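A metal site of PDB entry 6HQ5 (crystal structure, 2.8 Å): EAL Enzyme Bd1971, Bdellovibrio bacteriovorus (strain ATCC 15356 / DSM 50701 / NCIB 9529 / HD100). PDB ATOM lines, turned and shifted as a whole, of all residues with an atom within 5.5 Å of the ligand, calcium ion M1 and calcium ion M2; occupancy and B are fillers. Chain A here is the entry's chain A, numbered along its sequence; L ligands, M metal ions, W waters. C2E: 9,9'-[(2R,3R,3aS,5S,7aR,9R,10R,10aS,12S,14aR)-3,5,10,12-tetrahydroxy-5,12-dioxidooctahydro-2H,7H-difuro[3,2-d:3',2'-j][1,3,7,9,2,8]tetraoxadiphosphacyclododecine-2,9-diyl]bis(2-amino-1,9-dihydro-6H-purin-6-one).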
ATOM      1  N   LEU A 157       9.564  -5.367  32.733  1.00  0.00           N
ATOM      2  CA  LEU A 157       9.641  -6.178  31.500  1.00  0.00           C
ATOM      3  C   LEU A 157      11.078  -6.614  31.229  1.00  0.00           C
ATOM      4  O   LEU A 157      11.990  -5.793  31.235  1.00  0.00           O
ATOM      5  CB  LEU A 157       9.106  -5.415  30.280  1.00  0.00           C
ATOM      6  CG  LEU A 157       7.643  -4.955  30.280  1.00  0.00           C
ATOM      7  CD1 LEU A 157       7.255  -4.465  28.881  1.00  0.00           C
ATOM      8  CD2 LEU A 157       6.701  -6.069  30.725  1.00  0.00           C
ATOM      9  N   GLN A 160      13.469 -11.310  25.558  1.00  0.00           N
ATOM     10  CA  GLN A 160      14.201 -12.470  25.041  1.00  0.00           C
ATOM     11  C   GLN A 160      14.419 -12.367  23.538  1.00  0.00           C
ATOM     12  O   GLN A 160      13.450 -12.248  22.792  1.00  0.00           O
ATOM     13  CB  GLN A 160      13.465 -13.774  25.334  1.00  0.00           C
ATOM     14  CG  GLN A 160      14.251 -14.982  24.853  1.00  0.00           C
ATOM     15  CD  GLN A 160      13.623 -16.294  25.267  1.00  0.00           C
ATOM     16  OE1 GLN A 160      12.410 -16.462  25.175  1.00  0.00           O
ATOM     17  NE2 GLN A 160      14.449 -17.235  25.723  1.00  0.00           N
ATOM     18  N   GLU A 174      10.876 -10.871  22.358  1.00  0.00           N
ATOM     19  CA  GLU A 174       9.573 -10.983  23.028  1.00  0.00           C
ATOM     20  C   GLU A 174       9.655 -10.306  24.388  1.00  0.00           C
ATOM     21  O   GLU A 174      10.618 -10.505  25.127  1.00  0.00           O
ATOM     22  CB  GLU A 174       9.152 -12.453  23.209  1.00  0.00           C
ATOM     23  CG  GLU A 174       7.732 -12.610  23.765  1.00  0.00           C
ATOM     24  CD  GLU A 174       7.276 -14.057  23.940  1.00  0.00           C
ATOM     25  OE1 GLU A 174       8.123 -14.979  23.947  1.00  0.00           O
ATOM     26  OE2 GLU A 174       6.048 -14.279  24.067  1.00  0.00           O
ATOM     27  N   ALA A 175       8.629  -9.507  24.705  1.00  0.00           N
ATOM     28  CA  ALA A 175       8.526  -8.850  26.003  1.00  0.00           C
ATOM     29  C   ALA A 175       7.852  -9.788  27.002  1.00  0.00           C
ATOM     30  O   ALA A 175       6.784 -10.331  26.719  1.00  0.00           O
ATOM     31  CB  ALA A 175       7.745  -7.559  25.881  1.00  0.00           C
ATOM     32  N   LEU A 176       8.468  -9.967  28.167  1.00  0.00           N
ATOM     33  CA  LEU A 176       7.945 -10.865  29.193  1.00  0.00           C
ATOM     34  C   LEU A 176       7.886 -10.163  30.555  1.00  0.00           C
ATOM     35  O   LEU A 176       8.841  -9.508  30.973  1.00  0.00           O
ATOM     36  CB  LEU A 176       8.818 -12.117  29.288  1.00  0.00           C
ATOM     37  CG  LEU A 176       8.896 -12.944  27.990  1.00  0.00           C
ATOM     38  CD1 LEU A 176       9.990 -13.992  28.091  1.00  0.00           C
ATOM     39  CD2 LEU A 176       7.552 -13.580  27.684  1.00  0.00           C
ATOM     40  N   LEU A 177       6.747 -10.330  31.242  1.00  0.00           N
ATOM     41  CA  LEU A 177       6.490  -9.651  32.516  1.00  0.00           C
ATOM     42  C   LEU A 177       7.224 -10.332  33.656  1.00  0.00           C
ATOM     43  O   LEU A 177       7.402 -11.549  33.641  1.00  0.00           O
ATOM     44  CB  LEU A 177       4.990  -9.646  32.813  1.00  0.00           C
ATOM     45  CG  LEU A 177       4.521  -8.819  34.022  1.00  0.00           C
ATOM     46  CD1 LEU A 177       4.710  -7.327  33.748  1.00  0.00           C
ATOM     47  CD2 LEU A 177       3.065  -9.111  34.340  1.00  0.00           C
ATOM     48  N   ARG A 178       7.640  -9.544  34.635  1.00  0.00           N
ATOM     49  CA  ARG A 178       8.361 -10.060  35.810  1.00  0.00           C
ATOM     50  C   ARG A 178       7.880  -9.339  37.066  1.00  0.00           C
ATOM     51  O   ARG A 178       7.697  -8.113  37.053  1.00  0.00           O
ATOM     52  CB  ARG A 178       9.875  -9.859  35.638  1.00  0.00           C
ATOM     53  CG  ARG A 178      10.516 -10.725  34.562  1.00  0.00           C
ATOM     54  CD  ARG A 178      10.655 -12.149  35.037  1.00  0.00           C
ATOM     55  NE  ARG A 178      11.324 -13.015  34.073  1.00  0.00           N
ATOM     56  CZ  ARG A 178      10.733 -13.603  33.017  1.00  0.00           C
ATOM     57  NH1 ARG A 178       9.438 -13.429  32.765  1.00  0.00           N
ATOM     58  NH2 ARG A 178      11.451 -14.375  32.222  1.00  0.00           N
ATOM     59  N   PRO A 189       4.607 -19.154  39.132  1.00  0.00           N
ATOM     60  CA  PRO A 189       5.084 -18.391  37.977  1.00  0.00           C
ATOM     61  C   PRO A 189       3.982 -17.980  36.997  1.00  0.00           C
ATOM     62  O   PRO A 189       3.891 -16.806  36.632  1.00  0.00           O
ATOM     63  CB  PRO A 189       6.047 -19.354  37.281  1.00  0.00           C
ATOM     64  CG  PRO A 189       6.494 -20.315  38.315  1.00  0.00           C
ATOM     65  CD  PRO A 189       5.523 -20.259  39.463  1.00  0.00           C
ATOM     66  N   ILE A 193      -0.308 -14.334  36.328  1.00  0.00           N
ATOM     67  CA  ILE A 193      -0.774 -13.844  35.019  1.00  0.00           C
ATOM     68  C   ILE A 193      -2.233 -14.278  34.808  1.00  0.00           C
ATOM     69  O   ILE A 193      -3.043 -13.497  34.293  1.00  0.00           O
ATOM     70  CB  ILE A 193       0.098 -14.299  33.810  1.00  0.00           C
ATOM     71  CG1 ILE A 193       1.586 -13.956  33.968  1.00  0.00           C
ATOM     72  CG2 ILE A 193      -0.398 -13.643  32.522  1.00  0.00           C
ATOM     73  CD1 ILE A 193       2.422 -14.978  34.708  1.00  0.00           C
ATOM     74  N   GLU A 197      -5.099 -11.761  34.143  1.00  0.00           N
ATOM     75  CA  GLU A 197      -5.882 -11.920  32.919  1.00  0.00           C
ATOM     76  C   GLU A 197      -7.396 -12.092  33.122  1.00  0.00           C
ATOM     77  O   GLU A 197      -8.176 -11.658  32.284  1.00  0.00           O
ATOM     78  CB  GLU A 197      -5.336 -13.061  32.042  1.00  0.00           C
ATOM     79  CG  GLU A 197      -4.130 -12.655  31.213  1.00  0.00           C
ATOM     80  CD  GLU A 197      -3.691 -13.736  30.245  1.00  0.00           C
ATOM     81  OE1 GLU A 197      -4.129 -14.901  30.388  1.00  0.00           O
ATOM     82  OE2 GLU A 197      -2.879 -13.437  29.338  1.00  0.00           O
ATOM     83  N   ILE A 209       2.061  -2.243  30.175  1.00  0.00           N
ATOM     84  CA  ILE A 209       2.963  -3.175  29.485  1.00  0.00           C
ATOM     85  C   ILE A 209       3.242  -2.663  28.073  1.00  0.00           C
ATOM     86  O   ILE A 209       4.406  -2.492  27.687  1.00  0.00           O
ATOM     87  CB  ILE A 209       2.389  -4.600  29.436  1.00  0.00           C
ATOM     88  CG1 ILE A 209       2.426  -5.216  30.843  1.00  0.00           C
ATOM     89  CG2 ILE A 209       3.172  -5.472  28.469  1.00  0.00           C
ATOM     90  CD1 ILE A 209       1.689  -6.527  30.971  1.00  0.00           C
ATOM     91  N   ASN A 241       2.728  -9.723  24.375  1.00  0.00           N
ATOM     92  CA  ASN A 241       1.692 -10.702  24.693  1.00  0.00           C
ATOM     93  C   ASN A 241       0.400 -10.015  25.131  1.00  0.00           C
ATOM     94  O   ASN A 241       0.312  -9.497  26.236  1.00  0.00           O
ATOM     95  CB  ASN A 241       2.186 -11.654  25.789  1.00  0.00           C
ATOM     96  CG  ASN A 241       3.201 -12.659  25.276  1.00  0.00           C
ATOM     97  OD1 ASN A 241       2.945 -13.387  24.328  1.00  0.00           O
ATOM     98  ND2 ASN A 241       4.364 -12.702  25.918  1.00  0.00           N
ATOM     99  N   ILE A 242      -0.601 -10.017  24.248  1.00  0.00           N
ATOM    100  CA  ILE A 242      -1.893  -9.365  24.492  1.00  0.00           C
ATOM    101  C   ILE A 242      -2.940 -10.414  24.892  1.00  0.00           C
ATOM    102  O   ILE A 242      -3.216 -11.339  24.137  1.00  0.00           O
ATOM    103  CB  ILE A 242      -2.368  -8.593  23.243  1.00  0.00           C
ATOM    104  CG1 ILE A 242      -1.722  -7.199  23.179  1.00  0.00           C
ATOM    105  CG2 ILE A 242      -3.876  -8.392  23.234  1.00  0.00           C
ATOM    106  CD1 ILE A 242      -0.214  -7.192  23.244  1.00  0.00           C
ATOM    107  N   SER A 243      -3.516 -10.247  26.078  1.00  0.00           N
ATOM    108  CA  SER A 243      -4.524 -11.194  26.585  1.00  0.00           C
ATOM    109  C   SER A 243      -5.894 -11.044  25.917  1.00  0.00           C
ATOM    110  O   SER A 243      -6.164 -10.044  25.252  1.00  0.00           O
ATOM    111  CB  SER A 243      -4.696 -11.038  28.097  1.00  0.00           C
ATOM    112  OG  SER A 243      -5.472  -9.886  28.411  1.00  0.00           O
ATOM    113  N   GLN A 246      -8.238  -7.971  27.259  1.00  0.00           N
ATOM    114  CA  GLN A 246      -7.739  -6.648  26.880  1.00  0.00           C
ATOM    115  C   GLN A 246      -7.824  -6.424  25.375  1.00  0.00           C
ATOM    116  O   GLN A 246      -7.868  -5.281  24.918  1.00  0.00           O
ATOM    117  CB  GLN A 246      -6.308  -6.403  27.398  1.00  0.00           C
ATOM    118  CG  GLN A 246      -5.173  -7.032  26.590  1.00  0.00           C
ATOM    119  CD  GLN A 246      -3.802  -6.723  27.191  1.00  0.00           C
ATOM    120  OE1 GLN A 246      -3.219  -7.550  27.897  1.00  0.00           O
ATOM    121  NE2 GLN A 246      -3.271  -5.530  26.914  1.00  0.00           N
ATOM    122  N   GLU A 273       0.804 -10.589  19.956  1.00  0.00           N
ATOM    123  CA  GLU A 273       0.882 -12.031  20.177  1.00  0.00           C
ATOM    124  C   GLU A 273      -0.273 -12.551  21.048  1.00  0.00           C
ATOM    125  O   GLU A 273      -0.280 -12.337  22.261  1.00  0.00           O
ATOM    126  CB  GLU A 273       2.239 -12.380  20.796  1.00  0.00           C
ATOM    127  CG  GLU A 273       2.636 -13.834  20.673  1.00  0.00           C
ATOM    128  CD  GLU A 273       4.130 -14.064  20.812  1.00  0.00           C
ATOM    129  OE1 GLU A 273       4.921 -13.357  20.139  1.00  0.00           O
ATOM    130  OE2 GLU A 273       4.518 -14.961  21.581  1.00  0.00           O
ATOM    131  N   ASP A 302       0.379 -17.720  19.461  1.00  0.00           N
ATOM    132  CA  ASP A 302       1.239 -18.382  20.421  1.00  0.00           C
ATOM    133  C   ASP A 302       0.523 -19.604  20.993  1.00  0.00           C
ATOM    134  O   ASP A 302      -0.712 -19.645  21.025  1.00  0.00           O
ATOM    135  CB  ASP A 302       1.599 -17.400  21.543  1.00  0.00           C
ATOM    136  CG  ASP A 302       2.661 -17.938  22.504  1.00  0.00           C
ATOM    137  OD1 ASP A 302       3.357 -18.922  22.167  1.00  0.00           O
ATOM    138  OD2 ASP A 302       2.791 -17.351  23.596  1.00  0.00           O
ATOM    139  N   ASP A 303       1.298 -20.591  21.422  1.00  0.00           N
ATOM    140  CA  ASP A 303       0.755 -21.815  22.005  1.00  0.00           C
ATOM    141  C   ASP A 303      -0.201 -22.489  21.024  1.00  0.00           C
ATOM    142  O   ASP A 303      -1.331 -22.830  21.377  1.00  0.00           O
ATOM    143  CB  ASP A 303       0.066 -21.509  23.354  1.00  0.00           C
ATOM    144  CG  ASP A 303       1.005 -20.822  24.356  1.00  0.00           C
ATOM    145  OD1 ASP A 303       2.210 -21.168  24.403  1.00  0.00           O
ATOM    146  OD2 ASP A 303       0.544 -19.942  25.107  1.00  0.00           O
ATOM    147  N   LYS A 323       3.855 -19.692  16.461  1.00  0.00           N
ATOM    148  CA  LYS A 323       4.904 -20.250  17.312  1.00  0.00           C
ATOM    149  C   LYS A 323       4.706 -21.733  17.611  1.00  0.00           C
ATOM    150  O   LYS A 323       3.670 -22.118  18.141  1.00  0.00           O
ATOM    151  CB  LYS A 323       4.977 -19.493  18.634  1.00  0.00           C
ATOM    152  CG  LYS A 323       5.508 -18.072  18.527  1.00  0.00           C
ATOM    153  CD  LYS A 323       6.223 -17.652  19.804  1.00  0.00           C
ATOM    154  CE  LYS A 323       6.850 -16.278  19.684  1.00  0.00           C
ATOM    155  NZ  LYS A 323       7.365 -15.810  20.997  1.00  0.00           N
ATOM    156  N   ASP A 325       5.238 -24.308  20.128  1.00  0.00           N
ATOM    157  CA  ASP A 325       5.398 -24.147  21.564  1.00  0.00           C
ATOM    158  C   ASP A 325       6.528 -25.013  22.130  1.00  0.00           C
ATOM    159  O   ASP A 325       6.923 -26.013  21.530  1.00  0.00           O
ATOM    160  CB  ASP A 325       4.079 -24.492  22.267  1.00  0.00           C
ATOM    161  CG  ASP A 325       4.034 -24.020  23.704  1.00  0.00           C
ATOM    162  OD1 ASP A 325       4.096 -22.786  23.929  1.00  0.00           O
ATOM    163  OD2 ASP A 325       3.951 -24.886  24.605  1.00  0.00           O
ATOM    164  N   ARG A 326       7.055 -24.593  23.282  1.00  0.00           N
ATOM    165  CA  ARG A 326       8.063 -25.344  24.050  1.00  0.00           C
ATOM    166  C   ARG A 326       7.723 -26.830  24.163  1.00  0.00           C
ATOM    167  O   ARG A 326       8.578 -27.685  23.952  1.00  0.00           O
ATOM    168  CB  ARG A 326       8.164 -24.791  25.474  1.00  0.00           C
ATOM    169  CG  ARG A 326       8.758 -23.404  25.607  1.00  0.00           C
ATOM    170  CD  ARG A 326       8.793 -22.974  27.064  1.00  0.00           C
ATOM    171  NE  ARG A 326       7.482 -22.548  27.559  1.00  0.00           N
ATOM    172  CZ  ARG A 326       7.232 -22.132  28.796  1.00  0.00           C
ATOM    173  NH1 ARG A 326       8.211 -22.080  29.702  1.00  0.00           N
ATOM    174  NH2 ARG A 326       6.006 -21.767  29.146  1.00  0.00           N
ATOM    175  N   GLU A 359      10.166 -22.308  19.593  1.00  0.00           N
ATOM    176  CA  GLU A 359      10.232 -21.805  20.958  1.00  0.00           C
ATOM    177  C   GLU A 359      10.838 -22.856  21.867  1.00  0.00           C
ATOM    178  O   GLU A 359      10.595 -24.051  21.705  1.00  0.00           O
ATOM    179  CB  GLU A 359       8.814 -21.475  21.406  1.00  0.00           C
ATOM    180  CG  GLU A 359       8.650 -20.663  22.677  1.00  0.00           C
ATOM    181  CD  GLU A 359       7.181 -20.447  23.002  1.00  0.00           C
ATOM    182  OE1 GLU A 359       6.557 -21.295  23.689  1.00  0.00           O
ATOM    183  OE2 GLU A 359       6.636 -19.445  22.527  1.00  0.00           O
ATOM    184  N   GLY A 360      11.635 -22.418  22.837  1.00  0.00           N
ATOM    185  CA  GLY A 360      12.209 -23.321  23.842  1.00  0.00           C
ATOM    186  C   GLY A 360      13.370 -24.171  23.372  1.00  0.00           C
ATOM    187  O   GLY A 360      13.524 -25.301  23.832  1.00  0.00           O
ATOM    188  N   ILE A 361      14.206 -23.640  22.482  1.00  0.00           N
ATOM    189  CA  ILE A 361      15.397 -24.350  22.015  1.00  0.00           C
ATOM    190  C   ILE A 361      16.501 -24.262  23.081  1.00  0.00           C
ATOM    191  O   ILE A 361      16.961 -23.160  23.402  1.00  0.00           O
ATOM    192  CB  ILE A 361      15.942 -23.765  20.692  1.00  0.00           C
ATOM    193  CG1 ILE A 361      14.870 -23.833  19.591  1.00  0.00           C
ATOM    194  CG2 ILE A 361      17.177 -24.518  20.239  1.00  0.00           C
ATOM    195  CD1 ILE A 361      15.112 -22.901  18.435  1.00  0.00           C
ATOM    196  N   GLU A 362      16.923 -25.409  23.599  1.00  0.00           N
ATOM    197  CA  GLU A 362      17.974 -25.469  24.624  1.00  0.00           C
ATOM    198  C   GLU A 362      19.288 -26.128  24.177  1.00  0.00           C
ATOM    199  O   GLU A 362      20.316 -25.930  24.830  1.00  0.00           O
ATOM    200  CB  GLU A 362      17.436 -26.185  25.867  1.00  0.00           C
ATOM    201  CG  GLU A 362      16.343 -25.406  26.577  1.00  0.00           C
ATOM    202  CD  GLU A 362      15.820 -26.098  27.818  1.00  0.00           C
ATOM    203  OE1 GLU A 362      16.247 -27.226  28.118  1.00  0.00           O
ATOM    204  OE2 GLU A 362      14.979 -25.485  28.502  1.00  0.00           O
ATOM    205  N   GLN A 379      13.956 -19.203  19.254  1.00  0.00           N
ATOM    206  CA  GLN A 379      13.840 -18.562  20.561  1.00  0.00           C
ATOM    207  C   GLN A 379      14.103 -19.639  21.613  1.00  0.00           C
ATOM    208  O   GLN A 379      13.537 -20.725  21.540  1.00  0.00           O
ATOM    209  CB  GLN A 379      12.434 -17.972  20.712  1.00  0.00           C
ATOM    210  CG  GLN A 379      12.255 -17.031  21.895  1.00  0.00           C
ATOM    211  CD  GLN A 379      10.844 -16.461  21.988  1.00  0.00           C
ATOM    212  OE1 GLN A 379      10.050 -16.560  21.049  1.00  0.00           O
ATOM    213  NE2 GLN A 379      10.523 -15.863  23.131  1.00  0.00           N
ATOM    214  N   GLY A 380      14.968 -19.356  22.573  1.00  0.00           N
ATOM    215  CA  GLY A 380      15.336 -20.344  23.578  1.00  0.00           C
ATOM    216  C   GLY A 380      16.597 -20.006  24.357  1.00  0.00           C
ATOM    217  O   GLY A 380      17.311 -19.064  24.020  1.00  0.00           O
ATOM    218  N   TYR A 381      16.854 -20.792  25.404  1.00  0.00           N
ATOM    219  CA  TYR A 381      18.021 -20.579  26.262  1.00  0.00           C
ATOM    220  C   TYR A 381      19.329 -20.855  25.542  1.00  0.00           C
ATOM    221  O   TYR A 381      20.354 -20.278  25.892  1.00  0.00           O
ATOM    222  CB  TYR A 381      17.948 -21.441  27.536  1.00  0.00           C
ATOM    223  CG  TYR A 381      16.844 -21.086  28.527  1.00  0.00           C
ATOM    224  CD1 TYR A 381      16.171 -19.859  28.466  1.00  0.00           C
ATOM    225  CD2 TYR A 381      16.502 -21.966  29.550  1.00  0.00           C
ATOM    226  CE1 TYR A 381      15.172 -19.554  29.378  1.00  0.00           C
ATOM    227  CE2 TYR A 381      15.503 -21.661  30.462  1.00  0.00           C
ATOM    228  CZ  TYR A 381      14.845 -20.455  30.374  1.00  0.00           C
ATOM    229  OH  TYR A 381      13.859 -20.143  31.272  1.00  0.00           O
ATOM    230  N   LEU A 382      19.307 -21.740  24.543  1.00  0.00           N
ATOM    231  CA  LEU A 382      20.489 -21.988  23.711  1.00  0.00           C
ATOM    232  C   LEU A 382      21.107 -20.663  23.281  1.00  0.00           C
ATOM    233  O   LEU A 382      22.308 -20.458  23.411  1.00  0.00           O
ATOM    234  CB  LEU A 382      20.132 -22.797  22.468  1.00  0.00           C
ATOM    235  CG  LEU A 382      21.302 -23.133  21.519  1.00  0.00           C
ATOM    236  CD1 LEU A 382      22.214 -24.163  22.163  1.00  0.00           C
ATOM    237  CD2 LEU A 382      20.802 -23.622  20.179  1.00  0.00           C
ATOM    238  N   PRO A 386      15.578 -14.627  28.717  1.00  0.00           N
ATOM    239  CA  PRO A 386      15.126 -13.238  28.755  1.00  0.00           C
ATOM    240  C   PRO A 386      15.942 -12.421  29.746  1.00  0.00           C
ATOM    241  O   PRO A 386      16.303 -12.935  30.804  1.00  0.00           O
ATOM    242  CB  PRO A 386      13.659 -13.343  29.197  1.00  0.00           C
ATOM    243  CG  PRO A 386      13.490 -14.732  29.704  1.00  0.00           C
ATOM    244  CD  PRO A 386      14.486 -15.583  28.999  1.00  0.00           C
HETATM  245  P1  C2E L   1       7.749 -16.845  31.320  1.00  0.00           P
HETATM  246  O2P C2E L   1       7.760 -17.565  32.618  1.00  0.00           O
HETATM  247  O1P C2E L   1       8.501 -15.588  31.176  1.00  0.00           O
HETATM  248  O5' C2E L   1       6.231 -16.516  30.894  1.00  0.00           O
HETATM  249  C5' C2E L   1       5.260 -17.542  30.912  1.00  0.00           C
HETATM  250  C4' C2E L   1       3.986 -17.067  30.234  1.00  0.00           C
HETATM  251  O4' C2E L   1       3.518 -15.879  30.887  1.00  0.00           O
HETATM  252  C3' C2E L   1       4.253 -16.608  28.811  1.00  0.00           C
HETATM  253  O3' C2E L   1       4.451 -17.744  27.914  1.00  0.00           O
HETATM  254  C2' C2E L   1       2.975 -15.825  28.573  1.00  0.00           C
HETATM  255  O2' C2E L   1       1.868 -16.693  28.337  1.00  0.00           O
HETATM  256  C1' C2E L   1       2.760 -15.109  29.905  1.00  0.00           C
HETATM  257  N9  C2E L   1       3.253 -13.702  29.828  1.00  0.00           N
HETATM  258  C8  C2E L   1       4.508 -13.268  29.987  1.00  0.00           C
HETATM  259  N7  C2E L   1       4.515 -11.958  29.842  1.00  0.00           N
HETATM  260  C5  C2E L   1       3.270 -11.554  29.586  1.00  0.00           C
HETATM  261  C6  C2E L   1       2.753 -10.351  29.362  1.00  0.00           C
HETATM  262  O6  C2E L   1       3.458  -9.346  29.356  1.00  0.00           O
HETATM  263  N1  C2E L   1       1.384 -10.213  29.110  1.00  0.00           N
HETATM  264  C2  C2E L   1       0.599 -11.353  29.116  1.00  0.00           C
HETATM  265  N2  C2E L   1      -0.703 -11.256  28.887  1.00  0.00           N
HETATM  266  N3  C2E L   1       1.169 -12.546  29.349  1.00  0.00           N
HETATM  267  C4  C2E L   1       2.485 -12.644  29.575  1.00  0.00           C
HETATM  268  P11 C2E L   1       4.755 -17.588  26.314  1.00  0.00           P
HETATM  269  O21 C2E L   1       3.980 -18.619  25.576  1.00  0.00           O
HETATM  270  O11 C2E L   1       4.665 -16.176  25.877  1.00  0.00           O
HETATM  271  O5A C2E L   1       6.299 -18.105  26.181  1.00  0.00           O
HETATM  272  C5A C2E L   1       7.429 -17.479  26.783  1.00  0.00           C
HETATM  273  C4A C2E L   1       7.946 -18.383  27.911  1.00  0.00           C
HETATM  274  O4A C2E L   1       8.900 -19.389  27.415  1.00  0.00           O
HETATM  275  C3A C2E L   1       8.711 -17.539  28.929  1.00  0.00           C
HETATM  276  O3A C2E L   1       8.264 -17.917  30.251  1.00  0.00           O
HETATM  277  C2A C2E L   1      10.154 -17.913  28.711  1.00  0.00           C
HETATM  278  O2A C2E L   1      10.909 -17.770  29.946  1.00  0.00           O
HETATM  279  C1A C2E L   1      10.034 -19.379  28.322  1.00  0.00           C
HETATM  280  N91 C2E L   1      11.263 -19.905  27.640  1.00  0.00           N
HETATM  281  C81 C2E L   1      11.910 -19.268  26.669  1.00  0.00           C
HETATM  282  N71 C2E L   1      12.943 -20.009  26.288  1.00  0.00           N
HETATM  283  C51 C2E L   1      12.953 -21.113  27.027  1.00  0.00           C
HETATM  284  C61 C2E L   1      13.778 -22.164  27.029  1.00  0.00           C
HETATM  285  O61 C2E L   1      14.735 -22.235  26.252  1.00  0.00           O
HETATM  286  N11 C2E L   1      13.539 -23.209  27.925  1.00  0.00           N
HETATM  287  C21 C2E L   1      12.454 -23.123  28.783  1.00  0.00           C
HETATM  288  N21 C2E L   1      12.198 -24.102  29.642  1.00  0.00           N
HETATM  289  N31 C2E L   1      11.659 -22.045  28.735  1.00  0.00           N
HETATM  290  C41 C2E L   1      11.906 -21.045  27.866  1.00  0.00           C
HETATM  291 CA    CA M   1       4.436 -20.524  24.330  1.00  0.00          CA
HETATM  292 CA    CA M   2       4.020 -15.382  23.791  1.00  0.00          CA
HETATM  293  O   HOH W   1       5.775 -16.862  23.507  1.00  0.00           O
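The side-chain carboxylate (OE2) of Glu 197 sits at hydrogen-bond distance from a nitrogen (N2) of the ligand (3.1 Å).
NE2 of Gln 160 lies within hydrogen-bond range of N71 of the ligand, 3.2 Å away.
A nitrogen (N11) of the ligand is in hydrogen-bond range of the side-chain carboxylate (OE2) of Glu 362.
The guanidinium group of Arg 178 lies within salt-bridge range of an oxygen (O1P) of the ligand, at 2.8 Å.
A nitrogen (N1) of the ligand lies within hydrogen-bond range of the backbone carbonyl oxygen of Asn 241 (3.1 Å).
An oxygen (O4A) of the ligand sits at hydrogen-bond distance from the guanidinium group (NE) of Arg 326 (3.5 Å).
O61 of the ligand lies within hydrogen-bond range of N of Tyr 381, 2.7 Å away.
N of Leu 177 is in hydrogen-bond range of N7 of the ligand.
The side-chain carboxylate (OE1) of Glu 273 lies within salt-bridge range of the side-chain amino group (NZ) of Lys 323 (3.6 Å).
The backbone carbonyl oxygen (O) of Ile 361 is in hydrogen-bond range of the backbone NH (N) of Leu 382, 3.0 Å away.
The side-chain carboxylate (OE1) of Glu 174 sits at hydrogen-bond distance from the side-chain amide nitrogen (NE2) of Gln 379, 2.7 Å away.
The backbone carbonyl oxygen of Gln 160 lies within hydrogen-bond range of the backbone NH of Glu 174 (3.0 Å).
O of Glu 273 lies within hydrogen-bond range of N of Ile 242 (3.1 Å).
N of Gly 360 sits at hydrogen-bond distance from O of Gln 379, at 2.9 Å.
The side-chain carboxylate of Glu 359 lies close to the backbone NH of Arg 326, at 3.4 Å.
The side-chain amide oxygen (OE1) of Gln 160 lies within hydrogen-bond range of the side-chain amide nitrogen (NE2) of Gln 379.
CA of Leu 176 touches N7 of the ligand, 3.7 Å away.
Ile 193 touches the ligand.
Ile 209 touches the ligand (CD1 to O6, 3.7 Å).
Gly 360 touches the ligand (CA to O61, 3.7 Å).
O of Ile 361 touches O61 of the ligand, at 3.7 Å.
Gly 380 touches the ligand.
Pro 386 touches the ligand.
Hydrophobic or aromatic side chains within 4 Å of the ligand: Leu 176, Leu 177, Ile 193, Ile 209, Tyr 381 and Pro 386.
The nearest printed residue that does not touch the ligand is Ser 243 (4.1 Å).
Of the 30 residues printed, 4 come within 4 Å of calcium ion M1.
The nearest printed residue that does not touch calcium ion M2 is Lys 323 (4.4 Å).
Calcium ion M1 is bound by OD1 of Asp 303 (2.3 Å), O21 of the ligand (2.3 Å), OD1 of Asp 325 (2.3 Å), OE1 of Glu 359 (2.3 Å) and OD1 of Asp 302 (2.9 Å).
Slightly farther from calcium ion M1 lies OE2 of Glu 359 (3.0 Å).
Calcium ion M2 is bound by the side-chain carboxylate of Glu 273, water W1, an oxygen (O11) of the ligand, the side-chain carboxylate of Glu 174, the side-chain amide oxygen of Asn 241 and the side-chain carboxylate of Asp 302.
Calcium ion M2 has six donor atoms within binding distance.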
